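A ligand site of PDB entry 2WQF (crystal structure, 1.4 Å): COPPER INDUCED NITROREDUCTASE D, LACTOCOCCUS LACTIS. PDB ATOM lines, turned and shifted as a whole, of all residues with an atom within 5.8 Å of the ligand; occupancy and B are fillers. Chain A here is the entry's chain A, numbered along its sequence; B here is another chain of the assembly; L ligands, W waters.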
ATOM      1  N   ARG A  10       9.769   9.514  16.757  1.00  0.00           N
ATOM      2  CA  ARG A  10       8.938   9.894  15.624  1.00  0.00           C
ATOM      3  C   ARG A  10       8.577   8.618  14.853  1.00  0.00           C
ATOM      4  O   ARG A  10       9.471   7.869  14.436  1.00  0.00           O
ATOM      5  CB  ARG A  10       9.651  10.856  14.677  1.00  0.00           C
ATOM      6  CG  ARG A  10       8.796  11.270  13.474  1.00  0.00           C
ATOM      7  CD  ARG A  10       9.559  11.374  12.193  1.00  0.00           C
ATOM      8  NE  ARG A  10      10.268  10.137  11.953  1.00  0.00           N
ATOM      9  CZ  ARG A  10       9.720   9.005  11.495  1.00  0.00           C
ATOM     10  NH1 ARG A  10       8.460   8.971  11.071  1.00  0.00           N
ATOM     11  NH2 ARG A  10      10.471   7.914  11.416  1.00  0.00           N
ATOM     12  N   ARG A  11       7.281   8.373  14.712  1.00  0.00           N
ATOM     13  CA  ARG A  11       6.770   7.231  13.970  1.00  0.00           C
ATOM     14  C   ARG A  11       5.534   7.612  13.166  1.00  0.00           C
ATOM     15  O   ARG A  11       4.871   8.611  13.441  1.00  0.00           O
ATOM     16  CB  ARG A  11       6.423   6.068  14.901  1.00  0.00           C
ATOM     17  CG  ARG A  11       7.609   5.491  15.667  1.00  0.00           C
ATOM     18  CD  ARG A  11       8.637   4.808  14.772  1.00  0.00           C
ATOM     19  NE  ARG A  11       8.043   3.769  13.953  1.00  0.00           N
ATOM     20  CZ  ARG A  11       7.717   2.553  14.392  1.00  0.00           C
ATOM     21  NH1 ARG A  11       8.004   2.195  15.635  1.00  0.00           N
ATOM     22  NH2 ARG A  11       7.161   1.702  13.572  1.00  0.00           N
ATOM     23  N   THR A  12       5.221   6.776  12.182  1.00  0.00           N
ATOM     24  CA  THR A  12       3.960   6.857  11.473  1.00  0.00           C
ATOM     25  C   THR A  12       2.840   6.340  12.371  1.00  0.00           C
ATOM     26  O   THR A  12       2.834   5.181  12.808  1.00  0.00           O
ATOM     27  CB  THR A  12       4.027   6.052  10.161  1.00  0.00           C
ATOM     28  OG1 THR A  12       4.880   6.725   9.241  1.00  0.00           O
ATOM     29  CG2 THR A  12       2.652   5.905   9.531  1.00  0.00           C
ATOM     30  N   ILE A  13       1.914   7.235  12.675  1.00  0.00           N
ATOM     31  CA  ILE A  13       0.730   6.917  13.451  1.00  0.00           C
ATOM     32  C   ILE A  13      -0.499   7.174  12.611  1.00  0.00           C
ATOM     33  O   ILE A  13      -0.780   8.311  12.252  1.00  0.00           O
ATOM     34  CB  ILE A  13       0.646   7.801  14.732  1.00  0.00           C
ATOM     35  CG1 ILE A  13       1.923   7.688  15.571  1.00  0.00           C
ATOM     36  CG2 ILE A  13      -0.620   7.505  15.535  1.00  0.00           C
ATOM     37  CD1 ILE A  13       2.195   6.314  16.152  1.00  0.00           C
ATOM     38  N   TYR A  14      -1.233   6.115  12.319  1.00  0.00           N
ATOM     39  CA  TYR A  14      -2.443   6.230  11.513  1.00  0.00           C
ATOM     40  C   TYR A  14      -3.691   6.496  12.353  1.00  0.00           C
ATOM     41  O   TYR A  14      -4.635   7.121  11.855  1.00  0.00           O
ATOM     42  CB  TYR A  14      -2.653   4.965  10.666  1.00  0.00           C
ATOM     43  CG  TYR A  14      -1.623   4.868   9.539  1.00  0.00           C
ATOM     44  CD1 TYR A  14      -1.529   5.874   8.566  1.00  0.00           C
ATOM     45  CD2 TYR A  14      -0.725   3.809   9.475  1.00  0.00           C
ATOM     46  CE1 TYR A  14      -0.608   5.798   7.548  1.00  0.00           C
ATOM     47  CE2 TYR A  14       0.214   3.710   8.446  1.00  0.00           C
ATOM     48  CZ  TYR A  14       0.275   4.712   7.498  1.00  0.00           C
ATOM     49  OH  TYR A  14       1.206   4.607   6.470  1.00  0.00           O
ATOM     50  N   PHE A  92      -8.052   9.858   8.250  1.00  0.00           N
ATOM     51  CA  PHE A  92      -7.296  11.086   8.072  1.00  0.00           C
ATOM     52  C   PHE A  92      -8.115  12.259   8.576  1.00  0.00           C
ATOM     53  O   PHE A  92      -7.612  13.109   9.290  1.00  0.00           O
ATOM     54  CB  PHE A  92      -6.883  11.281   6.608  1.00  0.00           C
ATOM     55  CG  PHE A  92      -5.982  10.229   6.092  1.00  0.00           C
ATOM     56  CD1 PHE A  92      -4.921   9.783   6.844  1.00  0.00           C
ATOM     57  CD2 PHE A  92      -6.172   9.690   4.834  1.00  0.00           C
ATOM     58  CE1 PHE A  92      -4.068   8.807   6.360  1.00  0.00           C
ATOM     59  CE2 PHE A  92      -5.348   8.716   4.342  1.00  0.00           C
ATOM     60  CZ  PHE A  92      -4.293   8.264   5.105  1.00  0.00           C
ATOM     61  N   VAL A 135      10.102  16.191   7.846  1.00  0.00           N
ATOM     62  CA  VAL A 135      10.499  15.292   8.949  1.00  0.00           C
ATOM     63  C   VAL A 135      10.832  16.082  10.194  1.00  0.00           C
ATOM     64  O   VAL A 135      10.610  15.591  11.299  1.00  0.00           O
ATOM     65  CB  VAL A 135      11.646  14.283   8.589  1.00  0.00           C
ATOM     66  CG1 VAL A 135      11.230  13.433   7.424  1.00  0.00           C
ATOM     67  CG2 VAL A 135      12.975  15.003   8.316  1.00  0.00           C
ATOM     68  N   TRP A 138       7.506  16.760  11.696  1.00  0.00           N
ATOM     69  CA  TRP A 138       6.969  15.470  12.147  1.00  0.00           C
ATOM     70  C   TRP A 138       7.591  15.089  13.491  1.00  0.00           C
ATOM     71  O   TRP A 138       6.891  14.687  14.426  1.00  0.00           O
ATOM     72  CB  TRP A 138       7.299  14.433  11.061  1.00  0.00           C
ATOM     73  CG  TRP A 138       6.586  13.117  11.097  1.00  0.00           C
ATOM     74  CD1 TRP A 138       5.832  12.588  12.103  1.00  0.00           C
ATOM     75  CD2 TRP A 138       6.604  12.143  10.048  1.00  0.00           C
ATOM     76  NE1 TRP A 138       5.350  11.339  11.713  1.00  0.00           N
ATOM     77  CE2 TRP A 138       5.819  11.064  10.464  1.00  0.00           C
ATOM     78  CE3 TRP A 138       7.192  12.098   8.778  1.00  0.00           C
ATOM     79  CZ2 TRP A 138       5.632   9.934   9.660  1.00  0.00           C
ATOM     80  CZ3 TRP A 138       7.007  10.983   7.984  1.00  0.00           C
ATOM     81  CH2 TRP A 138       6.225   9.919   8.430  1.00  0.00           C
ATOM     82  N   ASN A 149       1.166  11.157  10.232  1.00  0.00           N
ATOM     83  CA  ASN A 149       1.500  10.322   9.067  1.00  0.00           C
ATOM     84  C   ASN A 149       1.561  11.218   7.831  1.00  0.00           C
ATOM     85  O   ASN A 149       0.940  12.278   7.798  1.00  0.00           O
ATOM     86  CB  ASN A 149       0.529   9.134   8.952  1.00  0.00           C
ATOM     87  CG  ASN A 149      -0.897   9.569   8.677  1.00  0.00           C
ATOM     88  OD1 ASN A 149      -1.243   9.924   7.570  1.00  0.00           O
ATOM     89  ND2 ASN A 149      -1.720   9.558   9.679  1.00  0.00           N
ATOM     90  N   LEU A 150       2.365  10.821   6.866  1.00  0.00           N
ATOM     91  CA  LEU A 150       2.646  11.624   5.704  1.00  0.00           C
ATOM     92  C   LEU A 150       2.009  11.024   4.450  1.00  0.00           C
ATOM     93  O   LEU A 150       2.322   9.906   4.051  1.00  0.00           O
ATOM     94  CB  LEU A 150       4.170  11.734   5.507  1.00  0.00           C
ATOM     95  CG  LEU A 150       4.631  12.636   4.353  1.00  0.00           C
ATOM     96  CD1 LEU A 150       4.254  14.072   4.605  1.00  0.00           C
ATOM     97  CD2 LEU A 150       6.124  12.486   4.139  1.00  0.00           C
ATOM     98  N   GLN A 151       1.103  11.790   3.842  1.00  0.00           N
ATOM     99  CA  GLN A 151       0.356  11.380   2.681  1.00  0.00           C
ATOM    100  C   GLN A 151       0.738  12.193   1.458  1.00  0.00           C
ATOM    101  O   GLN A 151       1.329  13.284   1.552  1.00  0.00           O
ATOM    102  CB  GLN A 151      -1.150  11.505   2.928  1.00  0.00           C
ATOM    103  CG  GLN A 151      -1.670  10.672   4.074  1.00  0.00           C
ATOM    104  CD  GLN A 151      -1.207   9.236   3.985  1.00  0.00           C
ATOM    105  OE1 GLN A 151      -1.250   8.629   2.927  1.00  0.00           O
ATOM    106  NE2 GLN A 151      -0.728   8.693   5.097  1.00  0.00           N
ATOM    107  N   HIS A 152       0.364  11.639   0.298  1.00  0.00           N
ATOM    108  CA  HIS A 152       0.654  12.221  -1.008  1.00  0.00           C
ATOM    109  C   HIS A 152      -0.536  12.137  -1.948  1.00  0.00           C
ATOM    110  O   HIS A 152      -0.606  11.278  -2.824  1.00  0.00           O
ATOM    111  CB  HIS A 152       1.905  11.569  -1.592  1.00  0.00           C
ATOM    112  CG  HIS A 152       3.120  11.824  -0.771  1.00  0.00           C
ATOM    113  ND1 HIS A 152       3.526  10.962   0.229  1.00  0.00           N
ATOM    114  CD2 HIS A 152       3.967  12.884  -0.730  1.00  0.00           C
ATOM    115  CE1 HIS A 152       4.613  11.458   0.812  1.00  0.00           C
ATOM    116  NE2 HIS A 152       4.876  12.640   0.270  1.00  0.00           N
ATOM    117  N   ALA A 186       2.283   2.844  17.000  1.00  0.00           N
ATOM    118  CA  ALA A 186       2.880   2.520  15.720  1.00  0.00           C
ATOM    119  C   ALA A 186       3.008   1.016  15.535  1.00  0.00           C
ATOM    120  O   ALA A 186       3.134   0.248  16.508  1.00  0.00           O
ATOM    121  CB  ALA A 186       4.280   3.149  15.605  1.00  0.00           C
ATOM    122  N   LYS A 189       8.446  -2.276  12.700  1.00  0.00           N
ATOM    123  CA  LYS A 189       9.316  -1.767  11.644  1.00  0.00           C
ATOM    124  C   LYS A 189      10.646  -2.481  11.688  1.00  0.00           C
ATOM    125  O   LYS A 189      11.216  -2.686  12.758  1.00  0.00           O
ATOM    126  CB  LYS A 189       9.522  -0.243  11.798  1.00  0.00           C
ATOM    127  CG  LYS A 189      10.371   0.367  10.720  1.00  0.00           C
ATOM    128  CD  LYS A 189      10.412   1.900  10.768  1.00  0.00           C
ATOM    129  CE  LYS A 189      11.048   2.423  12.015  1.00  0.00           C
ATOM    130  NZ  LYS A 189      11.409   3.854  11.836  1.00  0.00           N
ATOM    131  N   PHE B  36      17.133   5.832  12.099  1.00  0.00           N
ATOM    132  CA  PHE B  36      15.851   6.318  12.582  1.00  0.00           C
ATOM    133  C   PHE B  36      15.200   7.386  11.738  1.00  0.00           C
ATOM    134  O   PHE B  36      14.230   7.992  12.157  1.00  0.00           O
ATOM    135  CB  PHE B  36      15.978   6.758  14.031  1.00  0.00           C
ATOM    136  CG  PHE B  36      16.416   5.640  14.937  1.00  0.00           C
ATOM    137  CD1 PHE B  36      15.721   4.443  14.968  1.00  0.00           C
ATOM    138  CD2 PHE B  36      17.536   5.789  15.742  1.00  0.00           C
ATOM    139  CE1 PHE B  36      16.111   3.419  15.805  1.00  0.00           C
ATOM    140  CE2 PHE B  36      17.946   4.769  16.556  1.00  0.00           C
ATOM    141  CZ  PHE B  36      17.236   3.573  16.588  1.00  0.00           C
ATOM    142  N   SER B  37      15.705   7.557  10.528  1.00  0.00           N
ATOM    143  CA  SER B  37      15.091   8.465   9.545  1.00  0.00           C
ATOM    144  C   SER B  37      14.024   7.708   8.730  1.00  0.00           C
ATOM    145  O   SER B  37      14.260   6.580   8.278  1.00  0.00           O
ATOM    146  CB  SER B  37      16.141   8.992   8.573  1.00  0.00           C
ATOM    147  OG  SER B  37      17.066   9.845   9.217  1.00  0.00           O
ATOM    148  N   PRO B  38      12.877   8.336   8.511  1.00  0.00           N
ATOM    149  CA  PRO B  38      11.834   7.718   7.678  1.00  0.00           C
ATOM    150  C   PRO B  38      12.150   7.820   6.177  1.00  0.00           C
ATOM    151  O   PRO B  38      12.779   8.783   5.719  1.00  0.00           O
ATOM    152  CB  PRO B  38      10.611   8.533   8.012  1.00  0.00           C
ATOM    153  CG  PRO B  38      11.144   9.907   8.291  1.00  0.00           C
ATOM    154  CD  PRO B  38      12.482   9.683   8.969  1.00  0.00           C
ATOM    155  N   THR B  39      11.708   6.814   5.432  1.00  0.00           N
ATOM    156  CA  THR B  39      11.816   6.767   3.987  1.00  0.00           C
ATOM    157  C   THR B  39      10.532   6.169   3.457  1.00  0.00           C
ATOM    158  O   THR B  39       9.876   5.383   4.151  1.00  0.00           O
ATOM    159  CB  THR B  39      13.000   5.898   3.507  1.00  0.00           C
ATOM    160  OG1 THR B  39      12.956   4.610   4.134  1.00  0.00           O
ATOM    161  CG2 THR B  39      14.319   6.574   3.790  1.00  0.00           C
ATOM    162  N   ALA B  40      10.155   6.542   2.231  1.00  0.00           N
ATOM    163  CA  ALA B  40       8.910   6.045   1.643  1.00  0.00           C
ATOM    164  C   ALA B  40       8.912   4.519   1.661  1.00  0.00           C
ATOM    165  O   ALA B  40       9.892   3.869   1.243  1.00  0.00           O
ATOM    166  CB  ALA B  40       8.744   6.562   0.232  1.00  0.00           C
ATOM    167  N   PHE B  41       7.815   3.946   2.158  1.00  0.00           N
ATOM    168  CA  PHE B  41       7.625   2.493   2.201  1.00  0.00           C
ATOM    169  C   PHE B  41       8.760   1.770   2.937  1.00  0.00           C
ATOM    170  O   PHE B  41       9.012   0.580   2.708  1.00  0.00           O
ATOM    171  CB  PHE B  41       7.406   1.935   0.796  1.00  0.00           C
ATOM    172  N   ASN B  42       9.399   2.490   3.855  1.00  0.00           N
ATOM    173  CA  ASN B  42      10.543   1.944   4.593  1.00  0.00           C
ATOM    174  C   ASN B  42      11.599   1.392   3.651  1.00  0.00           C
ATOM    175  O   ASN B  42      12.269   0.412   3.977  1.00  0.00           O
ATOM    176  CB  ASN B  42      10.113   0.877   5.619  1.00  0.00           C
ATOM    177  CG  ASN B  42      11.156   0.639   6.676  1.00  0.00           C
ATOM    178  OD1 ASN B  42      11.880   1.569   7.065  1.00  0.00           O
ATOM    179  ND2 ASN B  42      11.265  -0.606   7.136  1.00  0.00           N
ATOM    180  N   TRP B 125      10.715  10.725  -3.831  1.00  0.00           N
ATOM    181  CA  TRP B 125      10.783  10.373  -2.417  1.00  0.00           C
ATOM    182  C   TRP B 125      12.202   9.993  -2.033  1.00  0.00           C
ATOM    183  O   TRP B 125      12.602  10.204  -0.892  1.00  0.00           O
ATOM    184  CB  TRP B 125       9.803   9.227  -2.111  1.00  0.00           C
ATOM    185  CG  TRP B 125       8.359   9.628  -2.242  1.00  0.00           C
ATOM    186  CD1 TRP B 125       7.842  10.886  -2.101  1.00  0.00           C
ATOM    187  CD2 TRP B 125       7.258   8.770  -2.538  1.00  0.00           C
ATOM    188  NE1 TRP B 125       6.469  10.852  -2.283  1.00  0.00           N
ATOM    189  CE2 TRP B 125       6.095   9.571  -2.551  1.00  0.00           C
ATOM    190  CE3 TRP B 125       7.141   7.403  -2.807  1.00  0.00           C
ATOM    191  CZ2 TRP B 125       4.836   9.048  -2.795  1.00  0.00           C
ATOM    192  CZ3 TRP B 125       5.889   6.887  -3.052  1.00  0.00           C
ATOM    193  CH2 TRP B 125       4.750   7.708  -3.057  1.00  0.00           C
ATOM    194  N   GLN B 128      13.989  13.296  -1.523  1.00  0.00           N
ATOM    195  CA  GLN B 128      13.559  13.798  -0.225  1.00  0.00           C
ATOM    196  C   GLN B 128      14.269  13.029   0.894  1.00  0.00           C
ATOM    197  O   GLN B 128      14.739  13.632   1.882  1.00  0.00           O
ATOM    198  CB  GLN B 128      12.023  13.707  -0.098  1.00  0.00           C
ATOM    199  CG  GLN B 128      11.329  14.651  -1.064  1.00  0.00           C
ATOM    200  CD  GLN B 128       9.825  14.502  -1.069  1.00  0.00           C
ATOM    201  OE1 GLN B 128       9.264  13.628  -0.420  1.00  0.00           O
ATOM    202  NE2 GLN B 128       9.163  15.361  -1.834  1.00  0.00           N
ATOM    203  N   GLY B 129      14.350  11.707   0.726  1.00  0.00           N
ATOM    204  CA  GLY B 129      15.040  10.825   1.660  1.00  0.00           C
ATOM    205  C   GLY B 129      16.491  11.210   1.881  1.00  0.00           C
ATOM    206  O   GLY B 129      17.019  11.138   2.991  1.00  0.00           O
ATOM    207  N   ILE B 132      16.564  14.224   4.061  1.00  0.00           N
ATOM    208  CA  ILE B 132      16.192  13.807   5.408  1.00  0.00           C
ATOM    209  C   ILE B 132      17.389  13.214   6.153  1.00  0.00           C
ATOM    210  O   ILE B 132      17.722  13.657   7.271  1.00  0.00           O
ATOM    211  CB  ILE B 132      15.046  12.785   5.323  1.00  0.00           C
ATOM    212  CG1 ILE B 132      13.740  13.495   4.926  1.00  0.00           C
ATOM    213  CG2 ILE B 132      14.847  12.031   6.637  1.00  0.00           C
ATOM    214  CD1 ILE B 132      12.643  12.530   4.462  1.00  0.00           C
HETATM  215  N1  LIG L   1       3.277   6.880   4.430  1.00  0.00           N
HETATM  216  C1  LIG L   1       1.891   6.861   3.937  1.00  0.00           C
HETATM  217  O1  LIG L   1       1.026   6.332   4.591  1.00  0.00           O
HETATM  218  N2  LIG L   1       1.615   7.400   2.635  1.00  0.00           N
HETATM  219  C2  LIG L   1       2.592   7.976   1.838  1.00  0.00           C
HETATM  220  O2  LIG L   1       2.283   8.502   0.812  1.00  0.00           O
HETATM  221  C3  LIG L   1       3.983   7.973   2.322  1.00  0.00           C
HETATM  222  N3  LIG L   1       4.968   8.447   1.638  1.00  0.00           N
HETATM  223  C4  LIG L   1       6.257   8.754   2.350  1.00  0.00           C
HETATM  224  C5  LIG L   1       7.258   9.632   1.670  1.00  0.00           C
HETATM  225  C6  LIG L   1       8.379   9.998   2.275  1.00  0.00           C
HETATM  226  C7  LIG L   1       9.370  10.859   1.516  1.00  0.00           C
HETATM  227  C8  LIG L   1       8.635   9.531   3.686  1.00  0.00           C
HETATM  228  C9  LIG L   1       9.875   9.992   4.417  1.00  0.00           C
HETATM  229  C10 LIG L   1       7.763   8.724   4.301  1.00  0.00           C
HETATM  230  C11 LIG L   1       6.488   8.310   3.612  1.00  0.00           C
HETATM  231  N4  LIG L   1       5.531   7.432   4.218  1.00  0.00           N
HETATM  232  C12 LIG L   1       4.246   7.395   3.676  1.00  0.00           C
HETATM  233  C13 LIG L   1       5.762   6.855   5.535  1.00  0.00           C
HETATM  234  C14 LIG L   1       6.822   5.761   5.478  1.00  0.00           C
HETATM  235  O3  LIG L   1       6.267   4.615   4.880  1.00  0.00           O
HETATM  236  C15 LIG L   1       7.313   5.515   6.899  1.00  0.00           C
HETATM  237  O4  LIG L   1       7.987   6.704   7.272  1.00  0.00           O
HETATM  238  C16 LIG L   1       8.302   4.332   6.942  1.00  0.00           C
HETATM  239  O5  LIG L   1       7.615   3.114   6.691  1.00  0.00           O
HETATM  240  C17 LIG L   1       9.021   4.241   8.285  1.00  0.00           C
HETATM  241  O6  LIG L   1       8.054   4.108   9.316  1.00  0.00           O
HETATM  242  P1  LIG L   1       7.983   5.227  10.506  1.00  0.00           P
HETATM  243  O7  LIG L   1       9.327   5.376  11.118  1.00  0.00           O
HETATM  244  O8  LIG L   1       7.506   6.588   9.875  1.00  0.00           O
HETATM  245  O9  LIG L   1       6.906   4.663  11.533  1.00  0.00           O
HETATM  246  O   HOH W   1       5.742   1.306   4.865  1.00  0.00           O
HETATM  247  O   HOH W   2       3.332   8.133   7.201  1.00  0.00           O
HETATM  248  O   HOH W   3       3.879   3.811   6.310  1.00  0.00           O
HETATM  249  O   HOH W   4       5.279   4.928   2.156  1.00  0.00           O
HETATM  250  O   HOH W   5      -0.808   9.005   0.187  1.00  0.00           O
HETATM  251  O   HOH W   6       6.047   2.329  11.109  1.00  0.00           O
HETATM  252  O   HOH W   7       6.562   1.333   8.637  1.00  0.00           O
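Trp 138 touches the ligand. CB of Pro 38 of chain B touches O4 of the ligand, 3.3 Å away. Thr 39 of chain B touches the ligand (O to C14, 3.4 Å). Ala 40 of chain B touches the ligand (N to C8, 3.7 Å). CD1 of Trp 125 of chain B touches C7 of the ligand (3.9 Å). OE1 of Gln 128 of chain B touches C7 of the ligand, at 3.4 Å. Ile 132 of chain B touches the ligand (CD1 to C9, 3.8 Å). 17 residues have an atom within 4 Å of the ligand: Arg 10, Arg 11, Thr 12, Tyr 14, Trp 138, Leu 150, Gln 151, His 152, Lys 189, Pro 38 of chain B, Thr 39 of chain B, Ala 40 of chain B, Phe 41 of chain B, Asn 42 of chain B, Trp 125 of chain B, Gln 128 of chain B and Ile 132 of chain B.
Water W6 lies within hydrogen-bond range of O9 of the ligand (2.5 Å) and NH2 of Arg 11 (2.8 Å). Water W3 lies within hydrogen-bond range of the side-chain hydroxyl of Tyr 14 (2.8 Å) and an oxygen (O3) of the ligand (2.9 Å). Water W4 lies within hydrogen-bond range of N of Phe 41 of chain B (2.7 Å) and O3 of the ligand (2.9 Å). Water W2 lies within hydrogen-bond range of the backbone NH of Leu 150 (2.9 Å), the side-chain hydroxyl of Thr 12 (2.9 Å) and a nitrogen (N1) of the ligand (3.0 Å). Water W5 lies within hydrogen-bond range of OE1 of Gln 151 (2.8 Å), N of His 152 (2.9 Å) and O2 of the ligand (3.2 Å).
The side-chain hydroxyl of Tyr 14 is in hydrogen-bond range of an oxygen (O1) of the ligand (2.6 Å). NZ of Lys 189 is in salt-bridge range of O7 of the ligand. The backbone NH (N) of Thr 12 is in hydrogen-bond range of an oxygen (O9) of the ligand (2.8 Å). The side-chain hydroxyl (OG1) of Thr 12 lies within hydrogen-bond range of an oxygen (O8) of the ligand, at 2.7 Å. An oxygen (O7) of the ligand is in salt-bridge range of the guanidinium group (NH2) of Arg 10, at 2.8 Å. A ring nitrogen (ND1) of His 152 sits at hydrogen-bond distance from an oxygen (O2) of the ligand (2.8 Å). The guanidinium group (NE) of Arg 11 is in salt-bridge range of an oxygen (O9) of the ligand (2.8 Å). O of Leu 150 sits close to N2 of the ligand (3.0 Å). An oxygen (O1) of the ligand lies within hydrogen-bond range of the side-chain amide nitrogen (NE2) of Gln 151 (3.0 Å). O3 of the ligand is in hydrogen-bond range of N of Phe 41 of chain B, 3.2 Å away. An oxygen (O5) of the ligand lies within hydrogen-bond range of the backbone NH of Asn 42 of chain B, at 3.4 Å.
NE2 of His 152 lies within hydrogen-bond range of NE1 of Trp 125 of chain B (3.5 Å). The indole nitrogen (NE1) of Trp 138 is in hydrogen-bond range of the backbone carbonyl oxygen (O) of Arg 11. NE2 of Gln 151 is in hydrogen-bond range of OD1 of Asn 149.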
